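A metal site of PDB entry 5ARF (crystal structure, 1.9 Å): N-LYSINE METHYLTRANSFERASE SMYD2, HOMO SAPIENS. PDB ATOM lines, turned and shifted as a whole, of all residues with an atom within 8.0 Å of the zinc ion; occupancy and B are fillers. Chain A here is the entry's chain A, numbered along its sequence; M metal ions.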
ATOM      1  N   HIS A  51     -34.584  14.589  -8.053  1.00  0.00           N
ATOM      2  CA  HIS A  51     -33.381  13.794  -8.382  1.00  0.00           C
ATOM      3  C   HIS A  51     -32.257  14.112  -7.375  1.00  0.00           C
ATOM      4  O   HIS A  51     -32.248  15.199  -6.814  1.00  0.00           O
ATOM      5  CB  HIS A  51     -32.886  14.095  -9.839  1.00  0.00           C
ATOM      6  CG  HIS A  51     -33.794  13.593 -10.928  1.00  0.00           C
ATOM      7  ND1 HIS A  51     -34.956  14.243 -11.291  1.00  0.00           N
ATOM      8  CD2 HIS A  51     -33.703  12.531 -11.757  1.00  0.00           C
ATOM      9  CE1 HIS A  51     -35.552  13.600 -12.283  1.00  0.00           C
ATOM     10  NE2 HIS A  51     -34.799  12.563 -12.597  1.00  0.00           N
ATOM     11  N   CYS A  52     -31.398  13.145  -7.089  1.00  0.00           N
ATOM     12  CA  CYS A  52     -30.210  13.350  -6.254  1.00  0.00           C
ATOM     13  C   CYS A  52     -29.307  14.365  -6.954  1.00  0.00           C
ATOM     14  O   CYS A  52     -28.881  14.142  -8.055  1.00  0.00           O
ATOM     15  CB  CYS A  52     -29.401  12.039  -6.055  1.00  0.00           C
ATOM     16  SG  CYS A  52     -27.998  12.033  -4.895  1.00  0.00           S
ATOM     17  N   GLU A  53     -28.982  15.436  -6.288  1.00  0.00           N
ATOM     18  CA  GLU A  53     -28.003  16.373  -6.865  1.00  0.00           C
ATOM     19  C   GLU A  53     -26.624  15.823  -7.177  1.00  0.00           C
ATOM     20  O   GLU A  53     -25.962  16.324  -8.063  1.00  0.00           O
ATOM     21  CB  GLU A  53     -27.943  17.635  -6.001  1.00  0.00           C
ATOM     22  CG  GLU A  53     -29.335  18.239  -6.079  1.00  0.00           C
ATOM     23  CD  GLU A  53     -29.387  19.711  -5.805  1.00  0.00           C
ATOM     24  OE1 GLU A  53     -28.369  20.365  -6.050  1.00  0.00           O
ATOM     25  OE2 GLU A  53     -30.478  20.170  -5.414  1.00  0.00           O
ATOM     26  N   TYR A  54     -26.237  14.745  -6.508  1.00  0.00           N
ATOM     27  CA  TYR A  54     -24.910  14.158  -6.728  1.00  0.00           C
ATOM     28  C   TYR A  54     -24.914  13.184  -7.921  1.00  0.00           C
ATOM     29  O   TYR A  54     -24.074  13.274  -8.847  1.00  0.00           O
ATOM     30  CB  TYR A  54     -24.379  13.475  -5.480  1.00  0.00           C
ATOM     31  CG  TYR A  54     -22.965  12.980  -5.719  1.00  0.00           C
ATOM     32  CD1 TYR A  54     -21.931  13.894  -6.006  1.00  0.00           C
ATOM     33  CD2 TYR A  54     -22.672  11.635  -5.735  1.00  0.00           C
ATOM     34  CE1 TYR A  54     -20.644  13.449  -6.262  1.00  0.00           C
ATOM     35  CE2 TYR A  54     -21.406  11.178  -5.974  1.00  0.00           C
ATOM     36  CZ  TYR A  54     -20.398  12.071  -6.246  1.00  0.00           C
ATOM     37  OH  TYR A  54     -19.136  11.579  -6.461  1.00  0.00           O
ATOM     38  N   CYS A  55     -25.843  12.257  -7.905  1.00  0.00           N
ATOM     39  CA  CYS A  55     -25.857  11.189  -8.895  1.00  0.00           C
ATOM     40  C   CYS A  55     -26.991  11.188  -9.891  1.00  0.00           C
ATOM     41  O   CYS A  55     -27.027  10.342 -10.770  1.00  0.00           O
ATOM     42  CB  CYS A  55     -25.778   9.840  -8.147  1.00  0.00           C
ATOM     43  SG  CYS A  55     -27.336   9.375  -7.361  1.00  0.00           S
ATOM     44  N   PHE A  56     -27.933  12.131  -9.778  1.00  0.00           N
ATOM     45  CA  PHE A  56     -29.053  12.265 -10.698  1.00  0.00           C
ATOM     46  C   PHE A  56     -30.128  11.169 -10.571  1.00  0.00           C
ATOM     47  O   PHE A  56     -31.088  11.148 -11.296  1.00  0.00           O
ATOM     48  CB  PHE A  56     -28.560  12.499 -12.166  1.00  0.00           C
ATOM     49  CG  PHE A  56     -28.040  13.914 -12.448  1.00  0.00           C
ATOM     50  CD1 PHE A  56     -27.367  14.667 -11.487  1.00  0.00           C
ATOM     51  CD2 PHE A  56     -28.174  14.465 -13.716  1.00  0.00           C
ATOM     52  CE1 PHE A  56     -26.907  15.964 -11.748  1.00  0.00           C
ATOM     53  CE2 PHE A  56     -27.631  15.729 -14.004  1.00  0.00           C
ATOM     54  CZ  PHE A  56     -26.980  16.469 -13.025  1.00  0.00           C
ATOM     55  N   THR A  57     -30.032  10.305  -9.558  1.00  0.00           N
ATOM     56  CA  THR A  57     -30.996   9.250  -9.432  1.00  0.00           C
ATOM     57  C   THR A  57     -32.266   9.835  -8.916  1.00  0.00           C
ATOM     58  O   THR A  57     -32.244  10.601  -7.954  1.00  0.00           O
ATOM     59  CB  THR A  57     -30.516   8.194  -8.452  1.00  0.00           C
ATOM     60  OG1 THR A  57     -29.295   7.612  -8.945  1.00  0.00           O
ATOM     61  CG2 THR A  57     -31.608   7.119  -8.206  1.00  0.00           C
ATOM     62  N   ARG A  58     -33.363   9.479  -9.545  1.00  0.00           N
ATOM     63  CA  ARG A  58     -34.670   9.894  -9.095  1.00  0.00           C
ATOM     64  C   ARG A  58     -35.184   9.019  -7.935  1.00  0.00           C
ATOM     65  O   ARG A  58     -35.280   7.816  -8.071  1.00  0.00           O
ATOM     66  CB  ARG A  58     -35.687   9.816 -10.228  1.00  0.00           C
ATOM     67  CG  ARG A  58     -37.036  10.302  -9.780  1.00  0.00           C
ATOM     68  CD  ARG A  58     -37.690  11.294 -10.738  1.00  0.00           C
ATOM     69  NE  ARG A  58     -39.070  10.900 -10.826  1.00  0.00           N
ATOM     70  CZ  ARG A  58     -39.477   9.831 -11.500  1.00  0.00           C
ATOM     71  NH1 ARG A  58     -38.584   9.108 -12.193  1.00  0.00           N
ATOM     72  NH2 ARG A  58     -40.761   9.491 -11.520  1.00  0.00           N
ATOM     73  N   LYS A  59     -35.603   9.668  -6.860  1.00  0.00           N
ATOM     74  CA  LYS A  59     -36.186   8.973  -5.732  1.00  0.00           C
ATOM     75  C   LYS A  59     -37.313   9.795  -5.163  1.00  0.00           C
ATOM     76  O   LYS A  59     -37.227  11.037  -5.136  1.00  0.00           O
ATOM     77  CB  LYS A  59     -35.135   8.771  -4.643  1.00  0.00           C
ATOM     78  CG  LYS A  59     -33.984   7.874  -5.053  1.00  0.00           C
ATOM     79  CD  LYS A  59     -32.828   7.888  -4.075  1.00  0.00           C
ATOM     80  CE  LYS A  59     -33.063   7.198  -2.769  1.00  0.00           C
ATOM     81  NZ  LYS A  59     -33.087   5.746  -3.036  1.00  0.00           N
ATOM     82  N   LEU A  62     -35.964  12.021  -0.661  1.00  0.00           N
ATOM     83  CA  LEU A  62     -34.541  12.293  -0.773  1.00  0.00           C
ATOM     84  C   LEU A  62     -34.225  12.870   0.542  1.00  0.00           C
ATOM     85  O   LEU A  62     -35.140  13.367   1.200  1.00  0.00           O
ATOM     86  CB  LEU A  62     -34.289  13.302  -1.883  1.00  0.00           C
ATOM     87  CG  LEU A  62     -34.038  12.889  -3.352  1.00  0.00           C
ATOM     88  CD1 LEU A  62     -33.432  11.485  -3.520  1.00  0.00           C
ATOM     89  CD2 LEU A  62     -35.235  13.156  -4.237  1.00  0.00           C
ATOM     90  N   PHE A  72     -31.026  18.022  -2.241  1.00  0.00           N
ATOM     91  CA  PHE A  72     -31.588  16.735  -1.964  1.00  0.00           C
ATOM     92  C   PHE A  72     -30.684  15.680  -2.514  1.00  0.00           C
ATOM     93  O   PHE A  72     -30.112  15.859  -3.610  1.00  0.00           O
ATOM     94  CB  PHE A  72     -32.947  16.649  -2.656  1.00  0.00           C
ATOM     95  CG  PHE A  72     -33.973  17.586  -2.081  1.00  0.00           C
ATOM     96  CD1 PHE A  72     -33.956  18.935  -2.412  1.00  0.00           C
ATOM     97  CD2 PHE A  72     -34.949  17.115  -1.204  1.00  0.00           C
ATOM     98  CE1 PHE A  72     -34.899  19.805  -1.875  1.00  0.00           C
ATOM     99  CE2 PHE A  72     -35.888  17.980  -0.636  1.00  0.00           C
ATOM    100  CZ  PHE A  72     -35.859  19.324  -0.986  1.00  0.00           C
ATOM    101  N   TYR A  73     -30.592  14.590  -1.773  1.00  0.00           N
ATOM    102  CA  TYR A  73     -29.622  13.525  -1.987  1.00  0.00           C
ATOM    103  C   TYR A  73     -30.172  12.145  -1.656  1.00  0.00           C
ATOM    104  O   TYR A  73     -31.074  12.019  -0.841  1.00  0.00           O
ATOM    105  CB  TYR A  73     -28.402  13.801  -1.118  1.00  0.00           C
ATOM    106  CG  TYR A  73     -27.704  15.108  -1.461  1.00  0.00           C
ATOM    107  CD1 TYR A  73     -26.931  15.221  -2.591  1.00  0.00           C
ATOM    108  CD2 TYR A  73     -27.836  16.217  -0.632  1.00  0.00           C
ATOM    109  CE1 TYR A  73     -26.289  16.408  -2.905  1.00  0.00           C
ATOM    110  CE2 TYR A  73     -27.227  17.408  -0.918  1.00  0.00           C
ATOM    111  CZ  TYR A  73     -26.410  17.497  -2.064  1.00  0.00           C
ATOM    112  OH  TYR A  73     -25.771  18.695  -2.350  1.00  0.00           O
ATOM    113  N   CYS A  74     -29.636  11.115  -2.318  1.00  0.00           N
ATOM    114  CA  CYS A  74     -29.991   9.711  -2.049  1.00  0.00           C
ATOM    115  C   CYS A  74     -29.788   9.301  -0.602  1.00  0.00           C
ATOM    116  O   CYS A  74     -30.538   8.495  -0.117  1.00  0.00           O
ATOM    117  CB  CYS A  74     -29.069   8.796  -2.846  1.00  0.00           C
ATOM    118  SG  CYS A  74     -29.318   8.730  -4.612  1.00  0.00           S
ATOM    119  N   ASN A  75     -28.735   9.833   0.017  1.00  0.00           N
ATOM    120  CA  ASN A  75     -28.140   9.390   1.275  1.00  0.00           C
ATOM    121  C   ASN A  75     -26.918  10.198   1.614  1.00  0.00           C
ATOM    122  O   ASN A  75     -26.409  10.976   0.791  1.00  0.00           O
ATOM    123  CB  ASN A  75     -27.680   7.946   1.194  1.00  0.00           C
ATOM    124  CG  ASN A  75     -26.793   7.663   0.012  1.00  0.00           C
ATOM    125  OD1 ASN A  75     -25.810   8.388  -0.284  1.00  0.00           O
ATOM    126  ND2 ASN A  75     -27.134   6.607  -0.710  1.00  0.00           N
ATOM    127  N   GLU A  77     -23.798   9.639   1.777  1.00  0.00           N
ATOM    128  CA  GLU A  77     -22.608   9.569   0.924  1.00  0.00           C
ATOM    129  C   GLU A  77     -22.753  10.466  -0.275  1.00  0.00           C
ATOM    130  O   GLU A  77     -21.810  11.162  -0.632  1.00  0.00           O
ATOM    131  CB  GLU A  77     -22.318   8.171   0.395  1.00  0.00           C
ATOM    132  CG  GLU A  77     -21.835   7.187   1.445  1.00  0.00           C
ATOM    133  CD  GLU A  77     -21.088   5.996   0.838  1.00  0.00           C
ATOM    134  OE1 GLU A  77     -19.925   6.214   0.421  1.00  0.00           O
ATOM    135  OE2 GLU A  77     -21.668   4.866   0.775  1.00  0.00           O
ATOM    136  N   CYS A  78     -23.915  10.416  -0.929  1.00  0.00           N
ATOM    137  CA  CYS A  78     -24.206  11.288  -2.094  1.00  0.00           C
ATOM    138  C   CYS A  78     -24.025  12.743  -1.701  1.00  0.00           C
ATOM    139  O   CYS A  78     -23.304  13.479  -2.381  1.00  0.00           O
ATOM    140  CB  CYS A  78     -25.599  11.048  -2.652  1.00  0.00           C
ATOM    141  SG  CYS A  78     -25.747   9.720  -3.869  1.00  0.00           S
ATOM    142  N   GLN A  79     -24.664  13.132  -0.583  1.00  0.00           N
ATOM    143  CA  GLN A  79     -24.508  14.467   0.010  1.00  0.00           C
ATOM    144  C   GLN A  79     -23.060  14.803   0.312  1.00  0.00           C
ATOM    145  O   GLN A  79     -22.574  15.852  -0.175  1.00  0.00           O
ATOM    146  CB  GLN A  79     -25.344  14.623   1.251  1.00  0.00           C
ATOM    147  CG  GLN A  79     -25.329  16.008   1.926  1.00  0.00           C
ATOM    148  CD  GLN A  79     -26.040  15.963   3.305  1.00  0.00           C
ATOM    149  OE1 GLN A  79     -26.357  17.013   3.909  1.00  0.00           O
ATOM    150  NE2 GLN A  79     -26.269  14.767   3.808  1.00  0.00           N
ATOM    151  N   GLU A  81     -20.418  13.636  -1.008  1.00  0.00           N
ATOM    152  CA  GLU A  81     -19.711  13.719  -2.280  1.00  0.00           C
ATOM    153  C   GLU A  81     -19.913  15.036  -3.052  1.00  0.00           C
ATOM    154  O   GLU A  81     -19.030  15.503  -3.808  1.00  0.00           O
ATOM    155  CB  GLU A  81     -20.124  12.533  -3.153  1.00  0.00           C
ATOM    156  CG  GLU A  81     -19.557  11.188  -2.718  1.00  0.00           C
ATOM    157  CD  GLU A  81     -18.062  11.282  -2.591  1.00  0.00           C
ATOM    158  OE1 GLU A  81     -17.431  11.807  -3.547  1.00  0.00           O
ATOM    159  OE2 GLU A  81     -17.544  10.957  -1.511  1.00  0.00           O
HETATM  160 ZN    ZN M   1     -27.262   9.757  -5.312  1.00  0.00          ZN
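Four residues have an atom within 4 Å of the zinc ion: Cys 52, Cys 55, Cys 74 and Cys 78.
The backbone NH (N) of Cys 52 lies within hydrogen-bond range of the backbone carbonyl oxygen (O) of Thr 57. SG of Cys 52 sits close to N of Tyr 54 (3.6 Å). The backbone NH (N) of Cys 78 is in hydrogen-bond range of the side-chain amide oxygen (OD1) of Asn 75. The side-chain sulfur (SG) of Cys 55 sits close to the side-chain hydroxyl (OG1) of Thr 57 (3.1 Å).
The zinc ion is bound by the side-chain sulfur (SG) of Cys 55 (2.1 Å), the side-chain sulfur (SG) of Cys 78 (2.1 Å), the side-chain sulfur (SG) of Cys 74 (2.4 Å) and the side-chain sulfur (SG) of Cys 52 (2.4 Å). The zinc ion has four donor atoms within binding distance.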
